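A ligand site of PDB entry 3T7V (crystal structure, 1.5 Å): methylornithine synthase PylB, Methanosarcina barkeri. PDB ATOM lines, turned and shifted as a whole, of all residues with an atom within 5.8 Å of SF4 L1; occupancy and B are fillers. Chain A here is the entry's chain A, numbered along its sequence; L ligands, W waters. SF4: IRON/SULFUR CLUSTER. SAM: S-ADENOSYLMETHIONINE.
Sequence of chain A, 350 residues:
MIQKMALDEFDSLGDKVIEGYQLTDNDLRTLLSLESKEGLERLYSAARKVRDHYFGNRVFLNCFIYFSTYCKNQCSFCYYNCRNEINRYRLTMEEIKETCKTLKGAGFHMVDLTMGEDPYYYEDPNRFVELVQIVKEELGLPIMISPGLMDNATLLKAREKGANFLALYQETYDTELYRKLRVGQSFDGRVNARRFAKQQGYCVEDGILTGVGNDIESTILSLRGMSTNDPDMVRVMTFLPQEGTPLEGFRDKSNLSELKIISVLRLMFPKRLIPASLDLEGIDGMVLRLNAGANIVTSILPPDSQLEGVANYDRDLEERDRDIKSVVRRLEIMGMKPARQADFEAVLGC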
ATOM      1  N   TYR A  66       8.385 -17.189  10.887  1.00  0.00           N
ATOM      2  CA  TYR A  66       7.982 -17.456  12.281  1.00  0.00           C
ATOM      3  C   TYR A  66       8.557 -16.297  13.079  1.00  0.00           C
ATOM      4  O   TYR A  66       9.754 -16.253  13.386  1.00  0.00           O
ATOM      5  CB  TYR A  66       8.612 -18.802  12.683  1.00  0.00           C
ATOM      6  CG  TYR A  66       8.016 -19.469  13.904  1.00  0.00           C
ATOM      7  CD1 TYR A  66       7.047 -18.919  14.705  1.00  0.00           C
ATOM      8  CD2 TYR A  66       8.506 -20.737  14.241  1.00  0.00           C
ATOM      9  CE1 TYR A  66       6.479 -19.604  15.769  1.00  0.00           C
ATOM     10  CE2 TYR A  66       7.973 -21.429  15.316  1.00  0.00           C
ATOM     11  CZ  TYR A  66       6.988 -20.838  16.063  1.00  0.00           C
ATOM     12  OH  TYR A  66       6.529 -21.607  17.138  1.00  0.00           O
ATOM     13  N   CYS A  71       4.913 -18.570  23.256  1.00  0.00           N
ATOM     14  CA  CYS A  71       3.529 -19.093  23.270  1.00  0.00           C
ATOM     15  C   CYS A  71       3.038 -19.242  24.696  1.00  0.00           C
ATOM     16  O   CYS A  71       3.770 -19.776  25.528  1.00  0.00           O
ATOM     17  CB  CYS A  71       3.466 -20.387  22.562  1.00  0.00           C
ATOM     18  SG  CYS A  71       1.696 -20.822  22.264  1.00  0.00           S
ATOM     19  N   LYS A  72       1.788 -18.876  24.908  1.00  0.00           N
ATOM     20  CA  LYS A  72       1.153 -19.057  26.215  1.00  0.00           C
ATOM     21  C   LYS A  72       0.403 -20.411  26.345  1.00  0.00           C
ATOM     22  O   LYS A  72      -0.100 -20.739  27.418  1.00  0.00           O
ATOM     23  CB  LYS A  72       0.244 -17.841  26.523  1.00  0.00           C
ATOM     24  CG  LYS A  72      -0.977 -17.714  25.623  1.00  0.00           C
ATOM     25  CD  LYS A  72      -1.459 -16.195  25.743  1.00  0.00           C
ATOM     26  CE  LYS A  72      -2.714 -16.002  24.869  1.00  0.00           C
ATOM     27  NZ  LYS A  72      -3.849 -16.618  25.562  1.00  0.00           N
ATOM     28  N   ASN A  73       0.236 -21.114  25.249  1.00  0.00           N
ATOM     29  CA  ASN A  73      -0.552 -22.389  25.234  1.00  0.00           C
ATOM     30  C   ASN A  73       0.348 -23.589  25.571  1.00  0.00           C
ATOM     31  O   ASN A  73       1.598 -23.474  25.612  1.00  0.00           O
ATOM     32  CB  ASN A  73      -1.205 -22.613  23.857  1.00  0.00           C
ATOM     33  CG  ASN A  73      -2.480 -21.841  23.657  1.00  0.00           C
ATOM     34  OD1 ASN A  73      -3.002 -21.832  22.470  1.00  0.00           O
ATOM     35  ND2 ASN A  73      -3.052 -21.319  24.716  1.00  0.00           N
ATOM     36  N   GLN A  74      -0.292 -24.719  25.797  1.00  0.00           N
ATOM     37  CA  GLN A  74       0.410 -25.897  26.352  1.00  0.00           C
ATOM     38  C   GLN A  74       0.143 -27.135  25.509  1.00  0.00           C
ATOM     39  O   GLN A  74      -0.119 -28.247  26.010  1.00  0.00           O
ATOM     40  CB  GLN A  74       0.209 -26.111  27.873  1.00  0.00           C
ATOM     41  CG  GLN A  74      -1.195 -26.256  28.206  1.00  0.00           C
ATOM     42  CD  GLN A  74      -1.341 -26.416  29.737  1.00  0.00           C
ATOM     43  OE1 GLN A  74      -0.757 -27.327  30.360  1.00  0.00           O
ATOM     44  NE2 GLN A  74      -1.944 -25.422  30.332  1.00  0.00           N
ATOM     45  N   CYS A  75       0.163 -26.975  24.198  1.00  0.00           N
ATOM     46  CA  CYS A  75      -0.019 -28.140  23.334  1.00  0.00           C
ATOM     47  C   CYS A  75       0.993 -29.230  23.635  1.00  0.00           C
ATOM     48  O   CYS A  75       2.175 -29.014  23.734  1.00  0.00           O
ATOM     49  CB  CYS A  75       0.077 -27.733  21.880  1.00  0.00           C
ATOM     50  SG  CYS A  75      -1.137 -26.498  21.356  1.00  0.00           S
ATOM     51  N   PHE A  77       2.115 -31.670  21.897  1.00  0.00           N
ATOM     52  CA  PHE A  77       2.929 -32.109  20.744  1.00  0.00           C
ATOM     53  C   PHE A  77       4.011 -31.067  20.341  1.00  0.00           C
ATOM     54  O   PHE A  77       4.900 -31.399  19.535  1.00  0.00           O
ATOM     55  CB  PHE A  77       2.024 -32.382  19.496  1.00  0.00           C
ATOM     56  CG  PHE A  77       1.124 -31.257  19.137  1.00  0.00           C
ATOM     57  CD1 PHE A  77       1.564 -30.226  18.274  1.00  0.00           C
ATOM     58  CD2 PHE A  77      -0.159 -31.183  19.693  1.00  0.00           C
ATOM     59  CE1 PHE A  77       0.708 -29.156  18.001  1.00  0.00           C
ATOM     60  CE2 PHE A  77      -1.055 -30.182  19.325  1.00  0.00           C
ATOM     61  CZ  PHE A  77      -0.590 -29.126  18.508  1.00  0.00           C
ATOM     62  N   CYS A  78       3.860 -29.793  20.816  1.00  0.00           N
ATOM     63  CA  CYS A  78       4.621 -28.742  20.192  1.00  0.00           C
ATOM     64  C   CYS A  78       5.824 -28.327  21.014  1.00  0.00           C
ATOM     65  O   CYS A  78       5.722 -28.109  22.216  1.00  0.00           O
ATOM     66  CB  CYS A  78       3.679 -27.524  20.087  1.00  0.00           C
ATOM     67  SG  CYS A  78       4.482 -26.131  19.247  1.00  0.00           S
ATOM     68  N   TYR A  79       6.968 -28.222  20.340  1.00  0.00           N
ATOM     69  CA  TYR A  79       8.211 -27.816  21.046  1.00  0.00           C
ATOM     70  C   TYR A  79       8.031 -26.459  21.736  1.00  0.00           C
ATOM     71  O   TYR A  79       8.734 -26.186  22.731  1.00  0.00           O
ATOM     72  CB  TYR A  79       9.293 -27.675  19.983  1.00  0.00           C
ATOM     73  CG  TYR A  79      10.694 -27.394  20.524  1.00  0.00           C
ATOM     74  CD1 TYR A  79      11.385 -28.395  21.265  1.00  0.00           C
ATOM     75  CD2 TYR A  79      11.242 -26.161  20.352  1.00  0.00           C
ATOM     76  CE1 TYR A  79      12.669 -28.115  21.747  1.00  0.00           C
ATOM     77  CE2 TYR A  79      12.534 -25.904  20.796  1.00  0.00           C
ATOM     78  CZ  TYR A  79      13.220 -26.893  21.485  1.00  0.00           C
ATOM     79  OH  TYR A  79      14.494 -26.606  21.935  1.00  0.00           O
ATOM     80  N   TYR A  80       7.179 -25.573  21.203  1.00  0.00           N
ATOM     81  CA  TYR A  80       7.130 -24.220  21.689  1.00  0.00           C
ATOM     82  C   TYR A  80       6.066 -24.047  22.775  1.00  0.00           C
ATOM     83  O   TYR A  80       5.848 -22.952  23.242  1.00  0.00           O
ATOM     84  CB  TYR A  80       6.870 -23.266  20.472  1.00  0.00           C
ATOM     85  CG  TYR A  80       7.982 -23.365  19.485  1.00  0.00           C
ATOM     86  CD1 TYR A  80       7.903 -24.220  18.387  1.00  0.00           C
ATOM     87  CD2 TYR A  80       9.108 -22.606  19.625  1.00  0.00           C
ATOM     88  CE1 TYR A  80       8.935 -24.375  17.492  1.00  0.00           C
ATOM     89  CE2 TYR A  80      10.174 -22.751  18.701  1.00  0.00           C
ATOM     90  CZ  TYR A  80      10.047 -23.665  17.633  1.00  0.00           C
ATOM     91  OH  TYR A  80      11.156 -23.718  16.801  1.00  0.00           O
ATOM     92  N   ASN A  81       5.475 -25.153  23.264  1.00  0.00           N
ATOM     93  CA  ASN A  81       4.515 -25.018  24.373  1.00  0.00           C
ATOM     94  C   ASN A  81       5.131 -24.299  25.562  1.00  0.00           C
ATOM     95  O   ASN A  81       6.346 -24.426  25.783  1.00  0.00           O
ATOM     96  CB  ASN A  81       3.787 -26.290  24.644  1.00  0.00           C
ATOM     97  CG  ASN A  81       4.500 -27.055  25.615  1.00  0.00           C
ATOM     98  OD1 ASN A  81       4.290 -26.833  26.856  1.00  0.00           O
ATOM     99  ND2 ASN A  81       5.329 -27.929  25.158  1.00  0.00           N
ATOM    100  N   CYS A  82       4.305 -23.606  26.304  1.00  0.00           N
ATOM    101  CA  CYS A  82       4.784 -22.713  27.330  1.00  0.00           C
ATOM    102  C   CYS A  82       5.541 -23.391  28.466  1.00  0.00           C
ATOM    103  O   CYS A  82       6.372 -22.690  29.137  1.00  0.00           O
ATOM    104  CB  CYS A  82       3.644 -21.935  27.840  1.00  0.00           C
ATOM    105  SG  CYS A  82       2.462 -22.783  28.845  1.00  0.00           S
ATOM    106  N   MET A 115       3.150 -17.060  14.491  1.00  0.00           N
ATOM    107  CA  MET A 115       3.672 -16.910  15.837  1.00  0.00           C
ATOM    108  C   MET A 115       3.053 -17.968  16.715  1.00  0.00           C
ATOM    109  O   MET A 115       1.989 -18.515  16.466  1.00  0.00           O
ATOM    110  CB  MET A 115       3.426 -15.490  16.451  1.00  0.00           C
ATOM    111  CG  MET A 115       1.926 -15.118  16.403  1.00  0.00           C
ATOM    112  SD  MET A 115       1.727 -13.589  17.393  1.00  0.00           S
ATOM    113  CE  MET A 115       0.017 -13.248  17.045  1.00  0.00           C
ATOM    114  N   GLY A 116       3.749 -18.214  17.839  1.00  0.00           N
ATOM    115  CA  GLY A 116       3.026 -18.786  19.001  1.00  0.00           C
ATOM    116  C   GLY A 116       1.988 -17.790  19.509  1.00  0.00           C
ATOM    117  O   GLY A 116       1.958 -16.640  18.988  1.00  0.00           O
ATOM    118  N   GLU A 117       1.151 -18.171  20.446  1.00  0.00           N
ATOM    119  CA  GLU A 117       0.216 -17.206  21.022  1.00  0.00           C
ATOM    120  C   GLU A 117       1.059 -16.377  21.997  1.00  0.00           C
ATOM    121  O   GLU A 117       1.076 -16.614  23.192  1.00  0.00           O
ATOM    122  CB  GLU A 117      -0.947 -17.920  21.717  1.00  0.00           C
ATOM    123  CG  GLU A 117      -1.812 -18.692  20.705  1.00  0.00           C
ATOM    124  CD  GLU A 117      -3.256 -18.829  21.179  1.00  0.00           C
ATOM    125  OE1 GLU A 117      -3.650 -18.295  22.215  1.00  0.00           O
ATOM    126  OE2 GLU A 117      -3.983 -19.518  20.367  1.00  0.00           O
ATOM    127  N   GLU A 171      -6.033 -29.955  13.918  1.00  0.00           N
ATOM    128  CA  GLU A 171      -5.169 -31.131  14.347  1.00  0.00           C
ATOM    129  C   GLU A 171      -5.927 -32.459  14.254  1.00  0.00           C
ATOM    130  O   GLU A 171      -5.446 -33.433  13.663  1.00  0.00           O
ATOM    131  CB  GLU A 171      -4.564 -31.058  15.747  1.00  0.00           C
ATOM    132  CG  GLU A 171      -3.988 -29.745  16.183  1.00  0.00           C
ATOM    133  CD  GLU A 171      -3.044 -29.175  15.191  1.00  0.00           C
ATOM    134  OE1 GLU A 171      -2.459 -29.833  14.261  1.00  0.00           O
ATOM    135  OE2 GLU A 171      -2.851 -27.958  15.293  1.00  0.00           O
ATOM    136  N   ARG A 182      -4.409 -30.330  21.910  1.00  0.00           N
ATOM    137  CA  ARG A 182      -4.562 -28.862  22.133  1.00  0.00           C
ATOM    138  C   ARG A 182      -5.130 -28.648  23.526  1.00  0.00           C
ATOM    139  O   ARG A 182      -6.298 -28.228  23.695  1.00  0.00           O
ATOM    140  CB  ARG A 182      -5.404 -28.197  21.031  1.00  0.00           C
ATOM    141  CG  ARG A 182      -4.492 -28.034  19.777  1.00  0.00           C
ATOM    142  CD  ARG A 182      -5.135 -27.080  18.753  1.00  0.00           C
ATOM    143  NE  ARG A 182      -4.167 -26.747  17.703  1.00  0.00           N
ATOM    144  CZ  ARG A 182      -3.198 -25.840  17.862  1.00  0.00           C
ATOM    145  NH1 ARG A 182      -3.207 -24.989  18.871  1.00  0.00           N
ATOM    146  NH2 ARG A 182      -2.298 -25.654  16.917  1.00  0.00           N
ATOM    147  N   GLN A 185      -7.712 -25.893  25.121  1.00  0.00           N
ATOM    148  CA  GLN A 185      -8.257 -25.048  24.082  1.00  0.00           C
ATOM    149  C   GLN A 185      -9.648 -25.564  23.675  1.00  0.00           C
ATOM    150  O   GLN A 185      -9.847 -26.776  23.651  1.00  0.00           O
ATOM    151  CB  GLN A 185      -7.316 -25.090  22.849  1.00  0.00           C
ATOM    152  CG  GLN A 185      -6.045 -24.361  23.238  1.00  0.00           C
ATOM    153  CD  GLN A 185      -4.952 -24.753  22.283  1.00  0.00           C
ATOM    154  OE1 GLN A 185      -5.116 -24.645  21.070  1.00  0.00           O
ATOM    155  NE2 GLN A 185      -3.852 -25.299  22.843  1.00  0.00           N
ATOM    156  N   ARG A 190     -11.881 -22.843  17.586  1.00  0.00           N
ATOM    157  CA  ARG A 190     -11.079 -22.765  16.340  1.00  0.00           C
ATOM    158  C   ARG A 190     -12.000 -22.858  15.143  1.00  0.00           C
ATOM    159  O   ARG A 190     -11.768 -22.191  14.126  1.00  0.00           O
ATOM    160  CB  ARG A 190      -9.954 -23.831  16.231  1.00  0.00           C
ATOM    161  CG  ARG A 190      -8.904 -23.653  17.313  1.00  0.00           C
ATOM    162  CD  ARG A 190      -7.852 -24.722  17.373  1.00  0.00           C
ATOM    163  NE  ARG A 190      -6.801 -24.557  16.370  1.00  0.00           N
ATOM    164  CZ  ARG A 190      -5.723 -23.778  16.513  1.00  0.00           C
ATOM    165  NH1 ARG A 190      -5.607 -22.905  17.570  1.00  0.00           N
ATOM    166  NH2 ARG A 190      -4.710 -23.810  15.607  1.00  0.00           N
ATOM    167  N   VAL A 310       8.570 -25.133  12.547  1.00  0.00           N
ATOM    168  CA  VAL A 310       7.782 -25.551  13.758  1.00  0.00           C
ATOM    169  C   VAL A 310       8.154 -26.967  14.181  1.00  0.00           C
ATOM    170  O   VAL A 310       8.462 -27.180  15.383  1.00  0.00           O
ATOM    171  CB  VAL A 310       6.234 -25.468  13.510  1.00  0.00           C
ATOM    172  CG1 VAL A 310       5.509 -25.880  14.807  1.00  0.00           C
ATOM    173  CG2 VAL A 310       5.911 -24.013  13.121  1.00  0.00           C
HETATM  174 FE1  SF4 L   1       0.697 -23.080  18.271  1.00  0.00          FE
HETATM  175 FE2  SF4 L   1       1.622 -22.642  20.865  1.00  0.00          FE
HETATM  176 FE3  SF4 L   1       2.701 -24.657  19.495  1.00  0.00          FE
HETATM  177 FE4  SF4 L   1       0.219 -24.866  20.381  1.00  0.00          FE
HETATM  178  S1  SF4 L   1       2.047 -24.666  21.697  1.00  0.00           S
HETATM  179  S2  SF4 L   1       0.941 -25.391  18.299  1.00  0.00           S
HETATM  180  S3  SF4 L   1      -0.602 -22.781  20.211  1.00  0.00           S
HETATM  181  S4  SF4 L   1       2.902 -22.491  18.984  1.00  0.00           S
HETATM  182  N   SAM L   2       0.469 -21.076  17.433  1.00  0.00           N
HETATM  183  CA  SAM L   2      -0.414 -21.077  16.360  1.00  0.00           C
HETATM  184  C   SAM L   2      -1.286 -22.260  16.277  1.00  0.00           C
HETATM  185  O   SAM L   2      -1.134 -23.211  17.083  1.00  0.00           O
HETATM  186  OXT SAM L   2      -2.254 -22.210  15.439  1.00  0.00           O
HETATM  187  CB  SAM L   2       0.202 -21.356  15.175  1.00  0.00           C
HETATM  188  CG  SAM L   2       1.251 -22.374  15.047  1.00  0.00           C
HETATM  189  SD  SAM L   2       0.893 -23.605  13.731  1.00  0.00           S
HETATM  190  CE  SAM L   2       2.212 -23.289  12.590  1.00  0.00           C
HETATM  191  C5' SAM L   2       1.462 -25.102  14.492  1.00  0.00           C
HETATM  192  C4' SAM L   2       0.856 -26.191  13.995  1.00  0.00           C
HETATM  193  O4' SAM L   2       2.284 -26.712  13.612  1.00  0.00           O
HETATM  194  C3' SAM L   2       0.135 -26.942  14.824  1.00  0.00           C
HETATM  195  O3' SAM L   2      -1.094 -26.538  14.199  1.00  0.00           O
HETATM  196  C2' SAM L   2       0.586 -28.236  14.145  1.00  0.00           C
HETATM  197  O2' SAM L   2      -0.338 -28.705  13.100  1.00  0.00           O
HETATM  198  C1' SAM L   2       2.017 -28.119  13.596  1.00  0.00           C
HETATM  199  N9  SAM L   2       2.990 -28.694  14.595  1.00  0.00           N
HETATM  200  C8  SAM L   2       3.366 -28.232  15.829  1.00  0.00           C
HETATM  201  N7  SAM L   2       4.213 -29.101  16.379  1.00  0.00           N
HETATM  202  C5  SAM L   2       4.399 -30.125  15.476  1.00  0.00           C
HETATM  203  C6  SAM L   2       5.106 -31.336  15.554  1.00  0.00           C
HETATM  204  N6  SAM L   2       5.825 -31.687  16.617  1.00  0.00           N
HETATM  205  N1  SAM L   2       5.113 -32.136  14.475  1.00  0.00           N
HETATM  206  C2  SAM L   2       4.384 -31.831  13.356  1.00  0.00           C
HETATM  207  N3  SAM L   2       3.592 -30.739  13.296  1.00  0.00           N
HETATM  208  C4  SAM L   2       3.631 -29.873  14.366  1.00  0.00           C
HETATM  209  O   HOH W   1      -3.284 -21.544  18.624  1.00  0.00           O
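The side-chain sulfur of Cys 71 sits close to the backbone NH of Asn 73.
ND2 of Asn 81 is in hydrogen-bond range of O of Cys 78 (3.0 Å).
The side-chain sulfur (SG) of Cys 78 sits close to the backbone NH (N) of Tyr 80 (3.4 Å).
The guanidinium group (NH1) of Arg 182 sits close to the side-chain sulfur (SG) of Cys 75, at 3.6 Å.
The side-chain sulfur of Cys 75 sits close to the side-chain amide nitrogen of Gln 185, 3.3 Å away.
The backbone carbonyl oxygen (O) of Asn 73 lies within hydrogen-bond range of the backbone NH (N) of Cys 82 (2.8 Å).
The side-chain amide oxygen (OE1) of Gln 185 lies within hydrogen-bond range of the guanidinium group (NH1) of Arg 182, at 2.9 Å.
NH2 of Arg 182 is in salt-bridge range of OE2 of Glu 171, 2.9 Å away.
An iron atom (FE1) of SF4 L1 is bound by a nitrogen (N) of SAM L2, at 2.2 Å.
Residues that only touch SF4 L1: Asn 81, Gly 116 and Phe 77.
Eight residues have an atom within 4 Å of SF4 L1: Cys 71, Asn 73, Cys 75, Phe 77, Cys 78, Asn 81, Gly 116 and Arg 182.
Along chain A the residues within 4 Å of SF4 L1 span positions 71 to 182.
The nearest printed residue that does not touch SF4 L1 is Tyr 66 (4.2 Å).
FE2 of SF4 L1 is bound by SG of Cys 71.
SG of Cys 78 binds FE3 of SF4 L1.
An iron atom (FE4) of SF4 L1 is bound by the side-chain sulfur (SG) of Cys 75, 2.3 Å away.
The side-chain amide oxygen (OD1) of Asn 73 lies close to a sulfur (S3) of SF4 L1, 3.4 Å away.
The guanidinium group (NH2) of Arg 182 sits close to a sulfur (S2) of SF4 L1 (3.5 Å).
An oxygen (OXT) of SAM L2 is in salt-bridge range of the guanidinium group (NH2) of Arg 182 (3.7 Å).
The backbone carbonyl oxygen (O) of Phe 77 lies within hydrogen-bond range of a nitrogen (N6) of SAM L2, 3.1 Å away.
N of SAM L2 sits close to O of Met 115, 3.1 Å away.
The side-chain carboxylate (OE2) of Glu 171 lies within hydrogen-bond range of an oxygen (O3') of SAM L2, 2.5 Å away.
NH2 of Arg 190 lies within salt-bridge range of OXT of SAM L2, at 2.9 Å.
Water W1 lies within hydrogen-bond range of OE2 of Glu 117, NH1 of Arg 190, S3 of SF4 L1, OXT of SAM L2 and NH1 of Arg 182.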
